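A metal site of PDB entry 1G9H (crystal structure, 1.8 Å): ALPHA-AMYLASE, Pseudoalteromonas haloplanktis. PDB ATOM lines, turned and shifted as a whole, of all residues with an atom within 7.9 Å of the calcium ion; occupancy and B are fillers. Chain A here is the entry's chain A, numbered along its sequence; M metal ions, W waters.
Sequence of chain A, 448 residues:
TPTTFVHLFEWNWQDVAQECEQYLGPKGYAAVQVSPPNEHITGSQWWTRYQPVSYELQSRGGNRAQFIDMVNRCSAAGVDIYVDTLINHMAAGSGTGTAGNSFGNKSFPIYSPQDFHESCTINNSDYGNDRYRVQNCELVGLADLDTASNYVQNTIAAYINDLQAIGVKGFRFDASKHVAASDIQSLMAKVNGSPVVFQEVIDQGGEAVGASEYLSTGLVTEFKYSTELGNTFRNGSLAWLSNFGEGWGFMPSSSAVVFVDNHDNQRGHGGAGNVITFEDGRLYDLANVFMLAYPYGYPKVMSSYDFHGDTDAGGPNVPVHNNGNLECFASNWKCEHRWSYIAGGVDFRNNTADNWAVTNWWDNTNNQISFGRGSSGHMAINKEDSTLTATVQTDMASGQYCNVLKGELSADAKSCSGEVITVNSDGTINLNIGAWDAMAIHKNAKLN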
ATOM      1  N   ILE A  87     -18.147 -20.308 -18.645  1.00  0.00           N
ATOM      2  CA  ILE A  87     -19.380 -19.967 -19.329  1.00  0.00           C
ATOM      3  C   ILE A  87     -19.310 -18.671 -20.144  1.00  0.00           C
ATOM      4  O   ILE A  87     -20.209 -18.377 -20.934  1.00  0.00           O
ATOM      5  CB  ILE A  87     -20.554 -19.848 -18.320  1.00  0.00           C
ATOM      6  CG1 ILE A  87     -20.250 -18.757 -17.287  1.00  0.00           C
ATOM      7  CG2 ILE A  87     -20.812 -21.182 -17.655  1.00  0.00           C
ATOM      8  CD1 ILE A  87     -21.484 -18.218 -16.583  1.00  0.00           C
ATOM      9  N   ASN A  88     -18.202 -17.948 -20.033  1.00  0.00           N
ATOM     10  CA  ASN A  88     -18.099 -16.666 -20.709  1.00  0.00           C
ATOM     11  C   ASN A  88     -17.333 -16.605 -22.025  1.00  0.00           C
ATOM     12  O   ASN A  88     -17.701 -15.825 -22.916  1.00  0.00           O
ATOM     13  CB  ASN A  88     -17.478 -15.644 -19.734  1.00  0.00           C
ATOM     14  CG  ASN A  88     -17.388 -14.246 -20.324  1.00  0.00           C
ATOM     15  OD1 ASN A  88     -18.408 -13.599 -20.559  1.00  0.00           O
ATOM     16  ND2 ASN A  88     -16.171 -13.752 -20.523  1.00  0.00           N
ATOM     17  N   HIS A  89     -16.312 -17.433 -22.163  1.00  0.00           N
ATOM     18  CA  HIS A  89     -15.457 -17.324 -23.333  1.00  0.00           C
ATOM     19  C   HIS A  89     -14.760 -18.596 -23.790  1.00  0.00           C
ATOM     20  O   HIS A  89     -14.884 -19.670 -23.162  1.00  0.00           O
ATOM     21  CB  HIS A  89     -14.383 -16.285 -22.993  1.00  0.00           C
ATOM     22  CG  HIS A  89     -13.702 -16.548 -21.675  1.00  0.00           C
ATOM     23  ND1 HIS A  89     -14.087 -15.926 -20.506  1.00  0.00           N
ATOM     24  CD2 HIS A  89     -12.709 -17.405 -21.326  1.00  0.00           C
ATOM     25  CE1 HIS A  89     -13.373 -16.388 -19.501  1.00  0.00           C
ATOM     26  NE2 HIS A  89     -12.530 -17.288 -19.974  1.00  0.00           N
ATOM     27  N   HIS A 117     -19.664 -12.539 -29.627  1.00  0.00           N
ATOM     28  CA  HIS A 117     -19.999 -11.123 -29.734  1.00  0.00           C
ATOM     29  C   HIS A 117     -18.871 -10.498 -30.574  1.00  0.00           C
ATOM     30  O   HIS A 117     -17.756 -11.030 -30.601  1.00  0.00           O
ATOM     31  CB  HIS A 117     -19.975 -10.458 -28.351  1.00  0.00           C
ATOM     32  CG  HIS A 117     -21.084 -10.881 -27.450  1.00  0.00           C
ATOM     33  ND1 HIS A 117     -20.882 -11.202 -26.124  1.00  0.00           N
ATOM     34  CD2 HIS A 117     -22.415 -11.019 -27.675  1.00  0.00           C
ATOM     35  CE1 HIS A 117     -22.032 -11.516 -25.563  1.00  0.00           C
ATOM     36  NE2 HIS A 117     -22.980 -11.420 -26.483  1.00  0.00           N
ATOM     37  N   ILE A 122     -12.408  -5.001 -22.977  1.00  0.00           N
ATOM     38  CA  ILE A 122     -12.925  -4.544 -21.700  1.00  0.00           C
ATOM     39  C   ILE A 122     -11.791  -3.739 -21.071  1.00  0.00           C
ATOM     40  O   ILE A 122     -10.708  -4.273 -20.857  1.00  0.00           O
ATOM     41  CB  ILE A 122     -13.263  -5.726 -20.745  1.00  0.00           C
ATOM     42  CG1 ILE A 122     -14.512  -6.463 -21.228  1.00  0.00           C
ATOM     43  CG2 ILE A 122     -13.486  -5.212 -19.322  1.00  0.00           C
ATOM     44  CD1 ILE A 122     -14.853  -7.682 -20.399  1.00  0.00           C
ATOM     45  N   TYR A 132     -22.479  -2.753 -20.476  1.00  0.00           N
ATOM     46  CA  TYR A 132     -22.558  -3.334 -21.805  1.00  0.00           C
ATOM     47  C   TYR A 132     -21.177  -3.854 -22.214  1.00  0.00           C
ATOM     48  O   TYR A 132     -21.065  -4.998 -22.653  1.00  0.00           O
ATOM     49  CB  TYR A 132     -23.045  -2.317 -22.848  1.00  0.00           C
ATOM     50  CG  TYR A 132     -23.118  -2.894 -24.252  1.00  0.00           C
ATOM     51  CD1 TYR A 132     -24.265  -3.566 -24.682  1.00  0.00           C
ATOM     52  CD2 TYR A 132     -22.029  -2.791 -25.129  1.00  0.00           C
ATOM     53  CE1 TYR A 132     -24.322  -4.136 -25.956  1.00  0.00           C
ATOM     54  CE2 TYR A 132     -22.074  -3.362 -26.396  1.00  0.00           C
ATOM     55  CZ  TYR A 132     -23.218  -4.027 -26.814  1.00  0.00           C
ATOM     56  OH  TYR A 132     -23.286  -4.576 -28.081  1.00  0.00           O
ATOM     57  N   ARG A 133     -20.144  -3.033 -22.035  1.00  0.00           N
ATOM     58  CA  ARG A 133     -18.781  -3.450 -22.382  1.00  0.00           C
ATOM     59  C   ARG A 133     -18.251  -4.561 -21.467  1.00  0.00           C
ATOM     60  O   ARG A 133     -17.583  -5.479 -21.926  1.00  0.00           O
ATOM     61  CB  ARG A 133     -17.818  -2.257 -22.393  1.00  0.00           C
ATOM     62  CG  ARG A 133     -18.062  -1.298 -23.551  1.00  0.00           C
ATOM     63  CD  ARG A 133     -17.026  -0.185 -23.574  1.00  0.00           C
ATOM     64  NE  ARG A 133     -15.705  -0.677 -23.955  1.00  0.00           N
ATOM     65  CZ  ARG A 133     -15.245  -0.695 -25.201  1.00  0.00           C
ATOM     66  NH1 ARG A 133     -14.031  -1.162 -25.455  1.00  0.00           N
ATOM     67  NH2 ARG A 133     -15.994  -0.247 -26.201  1.00  0.00           N
ATOM     68  N   VAL A 134     -18.599  -4.513 -20.175  1.00  0.00           N
ATOM     69  CA  VAL A 134     -18.151  -5.545 -19.231  1.00  0.00           C
ATOM     70  C   VAL A 134     -18.700  -6.920 -19.647  1.00  0.00           C
ATOM     71  O   VAL A 134     -17.984  -7.927 -19.584  1.00  0.00           O
ATOM     72  CB  VAL A 134     -18.614  -5.211 -17.753  1.00  0.00           C
ATOM     73  CG1 VAL A 134     -18.412  -6.414 -16.823  1.00  0.00           C
ATOM     74  CG2 VAL A 134     -17.814  -4.040 -17.209  1.00  0.00           C
ATOM     75  N   GLN A 135     -19.933  -6.957 -20.143  1.00  0.00           N
ATOM     76  CA  GLN A 135     -20.565  -8.219 -20.507  1.00  0.00           C
ATOM     77  C   GLN A 135     -20.548  -8.640 -21.984  1.00  0.00           C
ATOM     78  O   GLN A 135     -20.795  -9.802 -22.288  1.00  0.00           O
ATOM     79  CB  GLN A 135     -21.998  -8.256 -19.953  1.00  0.00           C
ATOM     80  CG  GLN A 135     -22.015  -8.042 -18.449  1.00  0.00           C
ATOM     81  CD  GLN A 135     -23.409  -8.132 -17.833  1.00  0.00           C
ATOM     82  OE1 GLN A 135     -24.422  -7.855 -18.490  1.00  0.00           O
ATOM     83  NE2 GLN A 135     -23.470  -8.543 -16.561  1.00  0.00           N
ATOM     84  N   ASN A 136     -20.225  -7.708 -22.887  1.00  0.00           N
ATOM     85  CA  ASN A 136     -20.184  -8.033 -24.304  1.00  0.00           C
ATOM     86  C   ASN A 136     -18.797  -7.964 -24.924  1.00  0.00           C
ATOM     87  O   ASN A 136     -18.564  -8.551 -25.989  1.00  0.00           O
ATOM     88  CB  ASN A 136     -21.188  -7.185 -25.082  1.00  0.00           C
ATOM     89  CG  ASN A 136     -22.612  -7.470 -24.666  1.00  0.00           C
ATOM     90  OD1 ASN A 136     -23.163  -8.501 -25.028  1.00  0.00           O
ATOM     91  ND2 ASN A 136     -23.189  -6.600 -23.852  1.00  0.00           N
ATOM     92  N   CYS A 137     -17.872  -7.260 -24.279  1.00  0.00           N
ATOM     93  CA  CYS A 137     -16.510  -7.173 -24.799  1.00  0.00           C
ATOM     94  C   CYS A 137     -15.621  -8.278 -24.231  1.00  0.00           C
ATOM     95  O   CYS A 137     -16.014  -9.045 -23.345  1.00  0.00           O
ATOM     96  CB  CYS A 137     -15.918  -5.777 -24.562  1.00  0.00           C
ATOM     97  SG  CYS A 137     -16.779  -4.458 -25.488  1.00  0.00           S
ATOM     98  N   GLU A 138     -14.395  -8.358 -24.745  1.00  0.00           N
ATOM     99  CA  GLU A 138     -13.448  -9.392 -24.369  1.00  0.00           C
ATOM    100  C   GLU A 138     -12.617  -9.139 -23.127  1.00  0.00           C
ATOM    101  O   GLU A 138     -12.021  -8.066 -22.932  1.00  0.00           O
ATOM    102  CB  GLU A 138     -12.509  -9.681 -25.556  1.00  0.00           C
ATOM    103  CG  GLU A 138     -13.281  -9.991 -26.827  1.00  0.00           C
ATOM    104  CD  GLU A 138     -12.401 -10.156 -28.060  1.00  0.00           C
ATOM    105  OE1 GLU A 138     -11.289  -9.604 -28.086  1.00  0.00           O
ATOM    106  OE2 GLU A 138     -12.848 -10.837 -29.016  1.00  0.00           O
ATOM    107  N   LEU A 139     -12.560 -10.170 -22.286  1.00  0.00           N
ATOM    108  CA  LEU A 139     -11.766 -10.156 -21.058  1.00  0.00           C
ATOM    109  C   LEU A 139     -10.354 -10.569 -21.503  1.00  0.00           C
ATOM    110  O   LEU A 139     -10.114 -11.727 -21.869  1.00  0.00           O
ATOM    111  CB  LEU A 139     -12.339 -11.178 -20.058  1.00  0.00           C
ATOM    112  CG  LEU A 139     -11.607 -11.351 -18.722  1.00  0.00           C
ATOM    113  CD1 LEU A 139     -11.627 -10.033 -17.953  1.00  0.00           C
ATOM    114  CD2 LEU A 139     -12.254 -12.482 -17.918  1.00  0.00           C
ATOM    115  N   LEU A 142      -9.987 -12.772 -24.628  1.00  0.00           N
ATOM    116  CA  LEU A 142     -10.671 -14.061 -24.696  1.00  0.00           C
ATOM    117  C   LEU A 142     -11.947 -13.904 -25.519  1.00  0.00           C
ATOM    118  O   LEU A 142     -12.732 -12.988 -25.273  1.00  0.00           O
ATOM    119  CB  LEU A 142     -10.976 -14.570 -23.290  1.00  0.00           C
ATOM    120  CG  LEU A 142      -9.708 -14.778 -22.439  1.00  0.00           C
ATOM    121  CD1 LEU A 142     -10.079 -15.020 -20.968  1.00  0.00           C
ATOM    122  CD2 LEU A 142      -8.889 -15.929 -22.988  1.00  0.00           C
ATOM    123  N   ALA A 143     -12.130 -14.773 -26.518  1.00  0.00           N
ATOM    124  CA  ALA A 143     -13.303 -14.722 -27.417  1.00  0.00           C
ATOM    125  C   ALA A 143     -14.589 -14.782 -26.602  1.00  0.00           C
ATOM    126  O   ALA A 143     -14.874 -15.795 -25.962  1.00  0.00           O
ATOM    127  CB  ALA A 143     -13.238 -15.866 -28.437  1.00  0.00           C
ATOM    128  N   ASP A 144     -15.359 -13.705 -26.644  1.00  0.00           N
ATOM    129  CA  ASP A 144     -16.575 -13.595 -25.856  1.00  0.00           C
ATOM    130  C   ASP A 144     -17.812 -14.243 -26.453  1.00  0.00           C
ATOM    131  O   ASP A 144     -18.409 -13.724 -27.387  1.00  0.00           O
ATOM    132  CB  ASP A 144     -16.834 -12.130 -25.534  1.00  0.00           C
ATOM    133  CG  ASP A 144     -17.644 -11.948 -24.266  1.00  0.00           C
ATOM    134  OD1 ASP A 144     -17.155 -12.308 -23.178  1.00  0.00           O
ATOM    135  OD2 ASP A 144     -18.772 -11.418 -24.357  1.00  0.00           O
ATOM    136  N   LEU A 145     -18.240 -15.362 -25.886  1.00  0.00           N
ATOM    137  CA  LEU A 145     -19.415 -16.094 -26.377  1.00  0.00           C
ATOM    138  C   LEU A 145     -20.711 -15.296 -26.353  1.00  0.00           C
ATOM    139  O   LEU A 145     -20.951 -14.497 -25.430  1.00  0.00           O
ATOM    140  CB  LEU A 145     -19.626 -17.379 -25.576  1.00  0.00           C
ATOM    141  CG  LEU A 145     -18.668 -18.564 -25.768  1.00  0.00           C
ATOM    142  CD1 LEU A 145     -18.794 -19.563 -24.614  1.00  0.00           C
ATOM    143  CD2 LEU A 145     -18.971 -19.224 -27.098  1.00  0.00           C
ATOM    144  N   ASP A 146     -21.553 -15.518 -27.343  1.00  0.00           N
ATOM    145  CA  ASP A 146     -22.843 -14.867 -27.365  1.00  0.00           C
ATOM    146  C   ASP A 146     -23.715 -15.756 -26.463  1.00  0.00           C
ATOM    147  O   ASP A 146     -24.338 -16.732 -26.914  1.00  0.00           O
ATOM    148  CB  ASP A 146     -23.414 -14.808 -28.782  1.00  0.00           C
ATOM    149  CG  ASP A 146     -24.797 -14.166 -28.839  1.00  0.00           C
ATOM    150  OD1 ASP A 146     -25.305 -13.670 -27.801  1.00  0.00           O
ATOM    151  OD2 ASP A 146     -25.376 -14.165 -29.926  1.00  0.00           O
ATOM    152  N   THR A 147     -23.718 -15.447 -25.172  1.00  0.00           N
ATOM    153  CA  THR A 147     -24.479 -16.222 -24.212  1.00  0.00           C
ATOM    154  C   THR A 147     -26.014 -16.079 -24.283  1.00  0.00           C
ATOM    155  O   THR A 147     -26.733 -16.738 -23.543  1.00  0.00           O
ATOM    156  CB  THR A 147     -23.925 -15.983 -22.794  1.00  0.00           C
ATOM    157  OG1 THR A 147     -23.781 -14.574 -22.577  1.00  0.00           O
ATOM    158  CG2 THR A 147     -22.553 -16.657 -22.654  1.00  0.00           C
ATOM    159  N   ALA A 175     -15.986 -16.281 -14.305  1.00  0.00           N
ATOM    160  CA  ALA A 175     -16.236 -14.986 -14.920  1.00  0.00           C
ATOM    161  C   ALA A 175     -17.724 -14.662 -15.084  1.00  0.00           C
ATOM    162  O   ALA A 175     -18.132 -14.122 -16.126  1.00  0.00           O
ATOM    163  CB  ALA A 175     -15.507 -14.921 -16.288  1.00  0.00           C
ATOM    164  N   SER A 176     -18.537 -14.957 -14.067  1.00  0.00           N
ATOM    165  CA  SER A 176     -19.971 -14.703 -14.139  1.00  0.00           C
ATOM    166  C   SER A 176     -20.376 -13.239 -14.324  1.00  0.00           C
ATOM    167  O   SER A 176     -21.413 -12.972 -14.915  1.00  0.00           O
ATOM    168  CB  SER A 176     -20.688 -15.278 -12.928  1.00  0.00           C
ATOM    169  OG  SER A 176     -20.665 -16.678 -12.985  1.00  0.00           O
ATOM    170  N   LYS A 177     -19.573 -12.307 -13.809  1.00  0.00           N
ATOM    171  CA  LYS A 177     -19.854 -10.884 -13.945  1.00  0.00           C
ATOM    172  C   LYS A 177     -19.903 -10.467 -15.427  1.00  0.00           C
ATOM    173  O   LYS A 177     -20.584  -9.511 -15.809  1.00  0.00           O
ATOM    174  CB  LYS A 177     -18.773 -10.045 -13.252  1.00  0.00           C
ATOM    175  CG  LYS A 177     -19.067  -8.556 -13.292  1.00  0.00           C
ATOM    176  CD  LYS A 177     -17.845  -7.710 -12.997  1.00  0.00           C
ATOM    177  CE  LYS A 177     -17.493  -7.744 -11.532  1.00  0.00           C
ATOM    178  NZ  LYS A 177     -16.254  -6.974 -11.298  1.00  0.00           N
ATOM    179  N   HIS A 178     -19.177 -11.214 -16.243  1.00  0.00           N
ATOM    180  CA  HIS A 178     -19.086 -10.945 -17.672  1.00  0.00           C
ATOM    181  C   HIS A 178     -20.218 -11.536 -18.494  1.00  0.00           C
ATOM    182  O   HIS A 178     -20.236 -11.415 -19.714  1.00  0.00           O
ATOM    183  CB  HIS A 178     -17.712 -11.384 -18.171  1.00  0.00           C
ATOM    184  CG  HIS A 178     -16.591 -10.696 -17.462  1.00  0.00           C
ATOM    185  ND1 HIS A 178     -16.156  -9.437 -17.820  1.00  0.00           N
ATOM    186  CD2 HIS A 178     -15.877 -11.041 -16.364  1.00  0.00           C
ATOM    187  CE1 HIS A 178     -15.229  -9.034 -16.971  1.00  0.00           C
ATOM    188  NE2 HIS A 178     -15.034  -9.986 -16.082  1.00  0.00           N
ATOM    189  N   VAL A 179     -21.177 -12.144 -17.804  1.00  0.00           N
ATOM    190  CA  VAL A 179     -22.341 -12.727 -18.463  1.00  0.00           C
ATOM    191  C   VAL A 179     -23.576 -12.153 -17.769  1.00  0.00           C
ATOM    192  O   VAL A 179     -23.652 -12.129 -16.535  1.00  0.00           O
ATOM    193  CB  VAL A 179     -22.347 -14.276 -18.349  1.00  0.00           C
ATOM    194  CG1 VAL A 179     -23.607 -14.850 -18.988  1.00  0.00           C
ATOM    195  CG2 VAL A 179     -21.103 -14.846 -18.983  1.00  0.00           C
ATOM    196  N   ALA A 180     -24.504 -11.610 -18.554  1.00  0.00           N
ATOM    197  CA  ALA A 180     -25.721 -11.036 -18.007  1.00  0.00           C
ATOM    198  C   ALA A 180     -26.431 -12.070 -17.131  1.00  0.00           C
ATOM    199  O   ALA A 180     -26.513 -13.241 -17.499  1.00  0.00           O
ATOM    200  CB  ALA A 180     -26.647 -10.578 -19.128  1.00  0.00           C
ATOM    201  N   ASP A 183     -28.911 -14.191 -18.844  1.00  0.00           N
ATOM    202  CA  ASP A 183     -28.379 -15.250 -19.699  1.00  0.00           C
ATOM    203  C   ASP A 183     -28.125 -16.492 -18.846  1.00  0.00           C
ATOM    204  O   ASP A 183     -28.364 -17.620 -19.290  1.00  0.00           O
ATOM    205  CB  ASP A 183     -27.069 -14.829 -20.367  1.00  0.00           C
ATOM    206  CG  ASP A 183     -27.274 -13.870 -21.540  1.00  0.00           C
ATOM    207  OD1 ASP A 183     -26.271 -13.390 -22.090  1.00  0.00           O
ATOM    208  OD2 ASP A 183     -28.438 -13.596 -21.903  1.00  0.00           O
HETATM  209 CA    CA M   1     -19.460 -11.913 -21.958  1.00  0.00          CA
HETATM  210  O   HOH W   1     -17.814 -10.121 -21.390  1.00  0.00           O
HETATM  211  O   HOH W   2     -21.892 -12.546 -22.350  1.00  0.00           O
HETATM  212  O   HOH W   3     -19.817 -14.138 -22.965  1.00  0.00           O
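The backbone carbonyl oxygen (O) of Asn 88 lies within hydrogen-bond range of the backbone NH (N) of Leu 145, 3.1 Å away. NE2 of Gln 135 is in hydrogen-bond range of O of Lys 177. A ring nitrogen (ND1) of His 89 lies within hydrogen-bond range of the side-chain amide nitrogen (ND2) of Asn 88 (3.0 Å). A ring nitrogen (ND1) of His 178 lies within hydrogen-bond range of the backbone carbonyl oxygen of Val 134. N of His 117 lies within hydrogen-bond range of O of Asp 144 (2.8 Å).
Of the 26 residues printed, 4 come within 4 Å of the calcium ion.
The calcium ion is bound by O of His 178 (2.4 Å), OD1 of Asn 88 (2.4 Å), water W3 (2.5 Å), water W1 (2.5 Å), O of Gln 135 (2.5 Å), water W2 (2.5 Å), OD2 of Asp 144 (2.5 Å) and OD1 of Asp 144 (2.6 Å). The calcium ion has eight donor atoms within binding distance.
Water W3 lies within hydrogen-bond range of the backbone carbonyl oxygen of Asn 88 (2.7 Å) and the backbone carbonyl oxygen of Leu 145 (2.7 Å).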
